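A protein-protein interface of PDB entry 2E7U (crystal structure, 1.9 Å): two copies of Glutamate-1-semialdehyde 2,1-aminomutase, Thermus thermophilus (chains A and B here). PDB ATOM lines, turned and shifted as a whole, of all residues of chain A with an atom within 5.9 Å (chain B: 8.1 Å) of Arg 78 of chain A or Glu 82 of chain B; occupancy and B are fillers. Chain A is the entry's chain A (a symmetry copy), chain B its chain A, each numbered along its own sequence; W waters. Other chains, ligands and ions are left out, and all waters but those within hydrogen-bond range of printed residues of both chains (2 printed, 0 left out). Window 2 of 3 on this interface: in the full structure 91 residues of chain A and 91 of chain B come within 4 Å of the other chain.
Among the printed residues, merely in contact across the chains: Arg 40 of chain A with Arg 83 of chain B (3.5 Å), Arg 40 of chain A with Phe 87 of chain B (3.6 Å), Gly 41 of chain A with Phe 87 of chain B (3.7 Å), Leu 74 of chain A with Leu 81 of chain B (3.6 Å), Leu 74 of chain A with Leu 85 of chain B (3.7 Å), Arg 78 of chain A with Leu 81 of chain B (3.96 Å), Leu 81 of chain A with Leu 74 of chain B (3.6 Å), Leu 81 of chain A with Arg 78 of chain B (3.97 Å) and Leu 81 of chain A with Leu 81 of chain B (3.3 Å).
The side-chain carboxylate of Glu 79 of chain B lies within salt-bridge range of the guanidinium group of Arg 83 of chain B (3.98 Å).
Water W2 lies within hydrogen-bond range of the backbone carbonyl oxygen of Gly 41 of chain A and the backbone carbonyl oxygen of Glu 82 of chain B. Water W1 lies within hydrogen-bond range of N of Ala 69 of chain A and N of Leu 85 of chain B.
NE of Arg 78 of chain B is in salt-bridge range of OE2 of Glu 82 of chain A, 2.5 Å away. The side-chain carboxylate of Glu 82 of chain B is in salt-bridge range of the guanidinium group of Arg 78 of chain A. O of Arg 83 of chain B is in hydrogen-bond range of N of Gly 41 of chain A, at 2.8 Å.
Printed residues of chain B within 4 Å of Gly 41 of chain A: Arg 83 and Phe 87. No residue of chain B comes within 4 Å of Ala 75 of chain A. Arg 78 of chain A touches just these residues of chain B: Leu 81 (3.96 Å) and Glu 82 (2.5 Å). Printed residues of chain A within 4 Å of Leu 81 of chain B: Leu 74 (3.6 Å), Arg 78 (3.96 Å) and Leu 81 (3.3 Å). Glu 82 of chain B touches just one residue of chain A: Arg 78. Printed residues of chain A within 4 Å of Leu 85 of chain B: Leu 74. Printed residues of chain A within 4 Å of Phe 87 of chain B: Arg 40 (3.6 Å) and Gly 41 (3.7 Å). The nearest residue of chain A that does not touch Glu 82 of chain B is Leu 74 of chain A (4.1 Å). The nearest printed residue of chain B that does not touch Leu 81 of chain A is Val 77 of chain B (4.2 Å).
Of the 14 printed residues of chain A, 6 touch a printed residue of chain B. Printed residues of chain A that touch a printed residue of chain B: Arg 40, Gly 41, Leu 74, Arg 78, Leu 81 and Glu 82. Hydrophobic or aromatic side chains of chain A that line the printed part of chain B: Leu 74 and Leu 81. Along chain A the printed residues that touch a printed residue of chain B span positions 40 to 82. Hydrophobic or aromatic side chains of chain B within 4 Å of the printed part of chain A: Leu 74, Leu 81, Leu 85 and Phe 87. Among the printed residues, Asp or Glu carboxylates within 4 Å of a Lys or Arg side-chain nitrogen of the other chain: Arg 78 of chain A with Glu 82 of chain B (2.5 Å) and Glu 82 of chain A with Arg 78 of chain B (2.5 Å).
Leu 74 of chain A touches Leu 81 of chain B, and with the chains exchanged Leu 81 of chain A touches Leu 74 of chain B. Arg 78 of chain A touches Leu 81 of chain B, and with the chains exchanged Leu 81 of chain A touches Arg 78 of chain B. Arg 78 of chain A touches Glu 82 of chain B, and with the chains exchanged Glu 82 of chain A touches Arg 78 of chain B. Leu 81 of chain B touches its own counterpart, Leu 81 of chain A.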
ATOM      1  N   ARG A  40      14.993 -12.587  16.651  1.00  0.00           N
ATOM      2  CA  ARG A  40      14.282 -12.919  17.878  1.00  0.00           C
ATOM      3  C   ARG A  40      13.126 -13.868  17.608  1.00  0.00           C
ATOM      4  O   ARG A  40      12.520 -13.846  16.532  1.00  0.00           O
ATOM      5  CB  ARG A  40      13.747 -11.636  18.526  1.00  0.00           C
ATOM      6  CG  ARG A  40      13.015 -11.836  19.848  1.00  0.00           C
ATOM      7  CD  ARG A  40      12.305 -10.547  20.268  1.00  0.00           C
ATOM      8  NE  ARG A  40      13.229  -9.422  20.398  1.00  0.00           N
ATOM      9  CZ  ARG A  40      14.048  -9.238  21.431  1.00  0.00           C
ATOM     10  NH1 ARG A  40      14.061 -10.104  22.439  1.00  0.00           N
ATOM     11  NH2 ARG A  40      14.864  -8.188  21.455  1.00  0.00           N
ATOM     12  N   GLY A  41      12.822 -14.697  18.599  1.00  0.00           N
ATOM     13  CA  GLY A  41      11.729 -15.635  18.464  1.00  0.00           C
ATOM     14  C   GLY A  41      11.056 -15.880  19.798  1.00  0.00           C
ATOM     15  O   GLY A  41      11.690 -15.811  20.857  1.00  0.00           O
ATOM     16  N   ALA A  69      12.262 -20.071  22.203  1.00  0.00           N
ATOM     17  CA  ALA A  69      12.563 -19.641  23.566  1.00  0.00           C
ATOM     18  C   ALA A  69      11.628 -20.134  24.666  1.00  0.00           C
ATOM     19  O   ALA A  69      11.107 -19.326  25.436  1.00  0.00           O
ATOM     20  CB  ALA A  69      12.623 -18.120  23.601  1.00  0.00           C
ATOM     21  N   PRO A  71      10.482 -20.986  28.084  1.00  0.00           N
ATOM     22  CA  PRO A  71      10.974 -20.571  29.405  1.00  0.00           C
ATOM     23  C   PRO A  71      11.742 -21.620  30.201  1.00  0.00           C
ATOM     24  O   PRO A  71      12.787 -21.320  30.774  1.00  0.00           O
ATOM     25  CB  PRO A  71       9.699 -20.133  30.132  1.00  0.00           C
ATOM     26  CG  PRO A  71       8.815 -19.670  29.018  1.00  0.00           C
ATOM     27  CD  PRO A  71       9.035 -20.727  27.967  1.00  0.00           C
ATOM     28  N   VAL A  73      13.225 -24.379  29.057  1.00  0.00           N
ATOM     29  CA  VAL A  73      14.434 -24.766  28.345  1.00  0.00           C
ATOM     30  C   VAL A  73      15.504 -23.692  28.534  1.00  0.00           C
ATOM     31  O   VAL A  73      16.653 -24.003  28.851  1.00  0.00           O
ATOM     32  CB  VAL A  73      14.150 -24.964  26.832  1.00  0.00           C
ATOM     33  CG1 VAL A  73      15.432 -25.351  26.097  1.00  0.00           C
ATOM     34  CG2 VAL A  73      13.094 -26.055  26.645  1.00  0.00           C
ATOM     35  N   LEU A  74      15.130 -22.428  28.350  1.00  0.00           N
ATOM     36  CA  LEU A  74      16.091 -21.346  28.520  1.00  0.00           C
ATOM     37  C   LEU A  74      16.618 -21.303  29.949  1.00  0.00           C
ATOM     38  O   LEU A  74      17.796 -21.020  30.170  1.00  0.00           O
ATOM     39  CB  LEU A  74      15.472 -19.991  28.170  1.00  0.00           C
ATOM     40  CG  LEU A  74      15.126 -19.708  26.704  1.00  0.00           C
ATOM     41  CD1 LEU A  74      14.806 -18.223  26.536  1.00  0.00           C
ATOM     42  CD2 LEU A  74      16.287 -20.090  25.820  1.00  0.00           C
ATOM     43  N   ALA A  75      15.749 -21.583  30.920  1.00  0.00           N
ATOM     44  CA  ALA A  75      16.166 -21.560  32.322  1.00  0.00           C
ATOM     45  C   ALA A  75      17.259 -22.592  32.575  1.00  0.00           C
ATOM     46  O   ALA A  75      18.235 -22.317  33.274  1.00  0.00           O
ATOM     47  CB  ALA A  75      14.973 -21.828  33.243  1.00  0.00           C
ATOM     48  N   ARG A  76      17.095 -23.786  32.007  1.00  0.00           N
ATOM     49  CA  ARG A  76      18.086 -24.833  32.193  1.00  0.00           C
ATOM     50  C   ARG A  76      19.423 -24.437  31.561  1.00  0.00           C
ATOM     51  O   ARG A  76      20.487 -24.701  32.131  1.00  0.00           O
ATOM     52  CB  ARG A  76      17.596 -26.154  31.592  1.00  0.00           C
ATOM     53  CG  ARG A  76      18.341 -27.376  32.115  1.00  0.00           C
ATOM     54  CD  ARG A  76      17.952 -27.663  33.562  1.00  0.00           C
ATOM     55  NE  ARG A  76      16.540 -28.020  33.666  1.00  0.00           N
ATOM     56  CZ  ARG A  76      16.061 -29.248  33.471  1.00  0.00           C
ATOM     57  NH1 ARG A  76      16.882 -30.244  33.171  1.00  0.00           N
ATOM     58  NH2 ARG A  76      14.756 -29.472  33.555  1.00  0.00           N
ATOM     59  N   VAL A  77      19.374 -23.805  30.390  1.00  0.00           N
ATOM     60  CA  VAL A  77      20.599 -23.380  29.718  1.00  0.00           C
ATOM     61  C   VAL A  77      21.275 -22.264  30.526  1.00  0.00           C
ATOM     62  O   VAL A  77      22.495 -22.266  30.682  1.00  0.00           O
ATOM     63  CB  VAL A  77      20.319 -22.874  28.280  1.00  0.00           C
ATOM     64  CG1 VAL A  77      21.619 -22.388  27.627  1.00  0.00           C
ATOM     65  CG2 VAL A  77      19.710 -23.998  27.444  1.00  0.00           C
ATOM     66  N   ARG A  78      20.482 -21.325  31.042  1.00  0.00           N
ATOM     67  CA  ARG A  78      21.016 -20.220  31.849  1.00  0.00           C
ATOM     68  C   ARG A  78      21.801 -20.758  33.041  1.00  0.00           C
ATOM     69  O   ARG A  78      22.903 -20.294  33.336  1.00  0.00           O
ATOM     70  CB  ARG A  78      19.895 -19.338  32.402  1.00  0.00           C
ATOM     71  CG  ARG A  78      19.116 -18.534  31.387  1.00  0.00           C
ATOM     72  CD  ARG A  78      18.178 -17.557  32.103  1.00  0.00           C
ATOM     73  NE  ARG A  78      17.178 -17.008  31.197  1.00  0.00           N
ATOM     74  CZ  ARG A  78      15.884 -17.303  31.243  1.00  0.00           C
ATOM     75  NH1 ARG A  78      15.424 -18.143  32.159  1.00  0.00           N
ATOM     76  NH2 ARG A  78      15.050 -16.764  30.366  1.00  0.00           N
ATOM     77  N   GLU A  79      21.213 -21.725  33.733  1.00  0.00           N
ATOM     78  CA  GLU A  79      21.843 -22.324  34.904  1.00  0.00           C
ATOM     79  C   GLU A  79      23.160 -23.002  34.547  1.00  0.00           C
ATOM     80  O   GLU A  79      24.185 -22.813  35.208  1.00  0.00           O
ATOM     81  CB  GLU A  79      20.901 -23.359  35.531  1.00  0.00           C
ATOM     82  CG  GLU A  79      21.506 -24.130  36.698  1.00  0.00           C
ATOM     83  CD  GLU A  79      20.621 -25.276  37.169  1.00  0.00           C
ATOM     84  OE1 GLU A  79      20.549 -26.310  36.467  1.00  0.00           O
ATOM     85  OE2 GLU A  79      19.991 -25.138  38.236  1.00  0.00           O
ATOM     86  N   THR A  80      23.128 -23.789  33.483  1.00  0.00           N
ATOM     87  CA  THR A  80      24.298 -24.532  33.041  1.00  0.00           C
ATOM     88  C   THR A  80      25.476 -23.683  32.566  1.00  0.00           C
ATOM     89  O   THR A  80      26.626 -23.963  32.909  1.00  0.00           O
ATOM     90  CB  THR A  80      23.905 -25.515  31.918  1.00  0.00           C
ATOM     91  OG1 THR A  80      22.898 -26.402  32.410  1.00  0.00           O
ATOM     92  CG2 THR A  80      25.109 -26.332  31.462  1.00  0.00           C
ATOM     93  N   LEU A  81      25.198 -22.643  31.787  1.00  0.00           N
ATOM     94  CA  LEU A  81      26.273 -21.818  31.263  1.00  0.00           C
ATOM     95  C   LEU A  81      27.127 -21.146  32.334  1.00  0.00           C
ATOM     96  O   LEU A  81      28.319 -20.932  32.124  1.00  0.00           O
ATOM     97  CB  LEU A  81      25.716 -20.773  30.293  1.00  0.00           C
ATOM     98  CG  LEU A  81      24.930 -19.560  30.790  1.00  0.00           C
ATOM     99  CD1 LEU A  81      25.892 -18.475  31.287  1.00  0.00           C
ATOM    100  CD2 LEU A  81      24.101 -19.013  29.634  1.00  0.00           C
ATOM    101  N   GLU A  82      26.536 -20.830  33.483  1.00  0.00           N
ATOM    102  CA  GLU A  82      27.300 -20.178  34.542  1.00  0.00           C
ATOM    103  C   GLU A  82      28.461 -21.042  35.032  1.00  0.00           C
ATOM    104  O   GLU A  82      29.475 -20.514  35.487  1.00  0.00           O
ATOM    105  CB  GLU A  82      26.400 -19.826  35.728  1.00  0.00           C
ATOM    106  CG  GLU A  82      25.326 -18.783  35.444  1.00  0.00           C
ATOM    107  CD  GLU A  82      25.888 -17.465  34.932  1.00  0.00           C
ATOM    108  OE1 GLU A  82      27.032 -17.105  35.289  1.00  0.00           O
ATOM    109  OE2 GLU A  82      25.172 -16.776  34.178  1.00  0.00           O
ATOM    110  N   LEU B  74      30.562 -15.004  28.794  1.00  0.00           N
ATOM    111  CA  LEU B  74      29.298 -15.499  29.324  1.00  0.00           C
ATOM    112  C   LEU B  74      28.204 -14.444  29.205  1.00  0.00           C
ATOM    113  O   LEU B  74      27.050 -14.772  28.929  1.00  0.00           O
ATOM    114  CB  LEU B  74      29.434 -15.918  30.790  1.00  0.00           C
ATOM    115  CG  LEU B  74      30.274 -17.158  31.115  1.00  0.00           C
ATOM    116  CD1 LEU B  74      30.037 -17.564  32.569  1.00  0.00           C
ATOM    117  CD2 LEU B  74      29.893 -18.291  30.194  1.00  0.00           C
ATOM    118  N   ARG B  76      27.833 -12.167  26.901  1.00  0.00           N
ATOM    119  CA  ARG B  76      27.355 -12.114  25.529  1.00  0.00           C
ATOM    120  C   ARG B  76      26.420 -13.289  25.232  1.00  0.00           C
ATOM    121  O   ARG B  76      25.407 -13.124  24.545  1.00  0.00           O
ATOM    122  CB  ARG B  76      28.530 -12.122  24.546  1.00  0.00           C
ATOM    123  CG  ARG B  76      28.162 -11.632  23.152  1.00  0.00           C
ATOM    124  CD  ARG B  76      27.923 -10.125  23.158  1.00  0.00           C
ATOM    125  NE  ARG B  76      29.145  -9.400  23.493  1.00  0.00           N
ATOM    126  CZ  ARG B  76      30.089  -9.076  22.612  1.00  0.00           C
ATOM    127  NH1 ARG B  76      29.950  -9.402  21.335  1.00  0.00           N
ATOM    128  NH2 ARG B  76      31.184  -8.443  23.013  1.00  0.00           N
ATOM    129  N   VAL B  77      26.753 -14.471  25.749  1.00  0.00           N
ATOM    130  CA  VAL B  77      25.914 -15.647  25.528  1.00  0.00           C
ATOM    131  C   VAL B  77      24.573 -15.473  26.254  1.00  0.00           C
ATOM    132  O   VAL B  77      23.525 -15.803  25.704  1.00  0.00           O
ATOM    133  CB  VAL B  77      26.602 -16.944  26.021  1.00  0.00           C
ATOM    134  CG1 VAL B  77      25.671 -18.146  25.820  1.00  0.00           C
ATOM    135  CG2 VAL B  77      27.904 -17.165  25.254  1.00  0.00           C
ATOM    136  N   ARG B  78      24.613 -14.951  27.480  1.00  0.00           N
ATOM    137  CA  ARG B  78      23.392 -14.723  28.263  1.00  0.00           C
ATOM    138  C   ARG B  78      22.423 -13.828  27.496  1.00  0.00           C
ATOM    139  O   ARG B  78      21.227 -14.109  27.420  1.00  0.00           O
ATOM    140  CB  ARG B  78      23.700 -14.027  29.591  1.00  0.00           C
ATOM    141  CG  ARG B  78      24.480 -14.833  30.601  1.00  0.00           C
ATOM    142  CD  ARG B  78      24.530 -14.087  31.939  1.00  0.00           C
ATOM    143  NE  ARG B  78      25.536 -14.649  32.832  1.00  0.00           N
ATOM    144  CZ  ARG B  78      26.667 -14.035  33.164  1.00  0.00           C
ATOM    145  NH1 ARG B  78      26.939 -12.832  32.682  1.00  0.00           N
ATOM    146  NH2 ARG B  78      27.530 -14.632  33.973  1.00  0.00           N
ATOM    147  N   GLU B  79      22.950 -12.741  26.946  1.00  0.00           N
ATOM    148  CA  GLU B  79      22.138 -11.791  26.194  1.00  0.00           C
ATOM    149  C   GLU B  79      21.506 -12.440  24.969  1.00  0.00           C
ATOM    150  O   GLU B  79      20.309 -12.294  24.706  1.00  0.00           O
ATOM    151  CB  GLU B  79      23.005 -10.608  25.742  1.00  0.00           C
ATOM    152  CG  GLU B  79      22.282  -9.608  24.848  1.00  0.00           C
ATOM    153  CD  GLU B  79      23.216  -8.559  24.263  1.00  0.00           C
ATOM    154  OE1 GLU B  79      23.991  -8.890  23.338  1.00  0.00           O
ATOM    155  OE2 GLU B  79      23.181  -7.405  24.736  1.00  0.00           O
ATOM    156  N   THR B  80      22.320 -13.171  24.224  1.00  0.00           N
ATOM    157  CA  THR B  80      21.868 -13.823  23.005  1.00  0.00           C
ATOM    158  C   THR B  80      20.815 -14.913  23.192  1.00  0.00           C
ATOM    159  O   THR B  80      19.842 -14.978  22.437  1.00  0.00           O
ATOM    160  CB  THR B  80      23.075 -14.418  22.247  1.00  0.00           C
ATOM    161  OG1 THR B  80      23.998 -13.368  21.948  1.00  0.00           O
ATOM    162  CG2 THR B  80      22.630 -15.075  20.945  1.00  0.00           C
ATOM    163  N   LEU B  81      20.995 -15.763  24.197  1.00  0.00           N
ATOM    164  CA  LEU B  81      20.056 -16.851  24.407  1.00  0.00           C
ATOM    165  C   LEU B  81      18.623 -16.400  24.675  1.00  0.00           C
ATOM    166  O   LEU B  81      17.681 -17.099  24.307  1.00  0.00           O
ATOM    167  CB  LEU B  81      20.545 -17.765  25.533  1.00  0.00           C
ATOM    168  CG  LEU B  81      20.482 -17.332  26.998  1.00  0.00           C
ATOM    169  CD1 LEU B  81      19.067 -17.537  27.550  1.00  0.00           C
ATOM    170  CD2 LEU B  81      21.467 -18.180  27.796  1.00  0.00           C
ATOM    171  N   GLU B  82      18.450 -15.235  25.291  1.00  0.00           N
ATOM    172  CA  GLU B  82      17.103 -14.754  25.582  1.00  0.00           C
ATOM    173  C   GLU B  82      16.279 -14.544  24.313  1.00  0.00           C
ATOM    174  O   GLU B  82      15.055 -14.665  24.343  1.00  0.00           O
ATOM    175  CB  GLU B  82      17.148 -13.447  26.374  1.00  0.00           C
ATOM    176  CG  GLU B  82      17.739 -13.553  27.775  1.00  0.00           C
ATOM    177  CD  GLU B  82      17.016 -14.560  28.657  1.00  0.00           C
ATOM    178  OE1 GLU B  82      15.797 -14.774  28.474  1.00  0.00           O
ATOM    179  OE2 GLU B  82      17.671 -15.129  29.553  1.00  0.00           O
ATOM    180  N   ARG B  83      16.946 -14.237  23.202  1.00  0.00           N
ATOM    181  CA  ARG B  83      16.245 -14.008  21.939  1.00  0.00           C
ATOM    182  C   ARG B  83      15.848 -15.293  21.222  1.00  0.00           C
ATOM    183  O   ARG B  83      15.032 -15.263  20.303  1.00  0.00           O
ATOM    184  CB  ARG B  83      17.103 -13.160  20.993  1.00  0.00           C
ATOM    185  CG  ARG B  83      17.287 -11.806  21.398  1.00  0.00           C
ATOM    186  CD  ARG B  83      18.128 -11.031  20.486  1.00  0.00           C
ATOM    187  NE  ARG B  83      18.602  -9.970  21.147  1.00  0.00           N
ATOM    188  CZ  ARG B  83      19.852  -9.773  21.562  1.00  0.00           C
ATOM    189  NH1 ARG B  83      20.842 -10.410  21.086  1.00  0.00           N
ATOM    190  NH2 ARG B  83      20.141  -8.766  22.337  1.00  0.00           N
ATOM    191  N   GLY B  84      16.428 -16.416  21.639  1.00  0.00           N
ATOM    192  CA  GLY B  84      16.125 -17.695  21.010  1.00  0.00           C
ATOM    193  C   GLY B  84      17.418 -18.458  20.770  1.00  0.00           C
ATOM    194  O   GLY B  84      18.445 -17.849  20.471  1.00  0.00           O
ATOM    195  N   LEU B  85      17.373 -19.781  20.885  1.00  0.00           N
ATOM    196  CA  LEU B  85      18.572 -20.606  20.710  1.00  0.00           C
ATOM    197  C   LEU B  85      18.996 -20.877  19.264  1.00  0.00           C
ATOM    198  O   LEU B  85      20.174 -21.142  19.002  1.00  0.00           O
ATOM    199  CB  LEU B  85      18.390 -21.945  21.436  1.00  0.00           C
ATOM    200  CG  LEU B  85      18.054 -21.865  22.931  1.00  0.00           C
ATOM    201  CD1 LEU B  85      17.974 -23.269  23.513  1.00  0.00           C
ATOM    202  CD2 LEU B  85      19.112 -21.041  23.661  1.00  0.00           C
ATOM    203  N   PHE B  87      17.588 -20.241  14.763  1.00  0.00           N
ATOM    204  CA  PHE B  87      16.610 -19.712  13.816  1.00  0.00           C
ATOM    205  C   PHE B  87      16.612 -20.385  12.447  1.00  0.00           C
ATOM    206  O   PHE B  87      15.589 -20.406  11.769  1.00  0.00           O
ATOM    207  CB  PHE B  87      16.823 -18.207  13.635  1.00  0.00           C
ATOM    208  CG  PHE B  87      16.681 -17.429  14.905  1.00  0.00           C
ATOM    209  CD1 PHE B  87      15.433 -17.273  15.502  1.00  0.00           C
ATOM    210  CD2 PHE B  87      17.802 -16.914  15.545  1.00  0.00           C
ATOM    211  CE1 PHE B  87      15.304 -16.617  16.726  1.00  0.00           C
ATOM    212  CE2 PHE B  87      17.685 -16.258  16.770  1.00  0.00           C
ATOM    213  CZ  PHE B  87      16.431 -16.112  17.361  1.00  0.00           C
ATOM    214  N   LEU B 304      24.267 -18.582  19.830  1.00  0.00           N
ATOM    215  CA  LEU B 304      25.083 -18.596  21.041  1.00  0.00           C
ATOM    216  C   LEU B 304      26.572 -18.801  20.752  1.00  0.00           C
ATOM    217  O   LEU B 304      27.423 -18.151  21.365  1.00  0.00           O
ATOM    218  CB  LEU B 304      24.590 -19.670  22.018  1.00  0.00           C
ATOM    219  CG  LEU B 304      23.336 -19.353  22.845  1.00  0.00           C
ATOM    220  CD1 LEU B 304      22.106 -19.281  21.943  1.00  0.00           C
ATOM    221  CD2 LEU B 304      23.148 -20.430  23.906  1.00  0.00           C
HETATM  222  O   HOH W   1      14.741 -21.215  21.175  1.00  0.00           O
HETATM  223  O   HOH W   2      12.682 -14.450  22.973  1.00  0.00           O
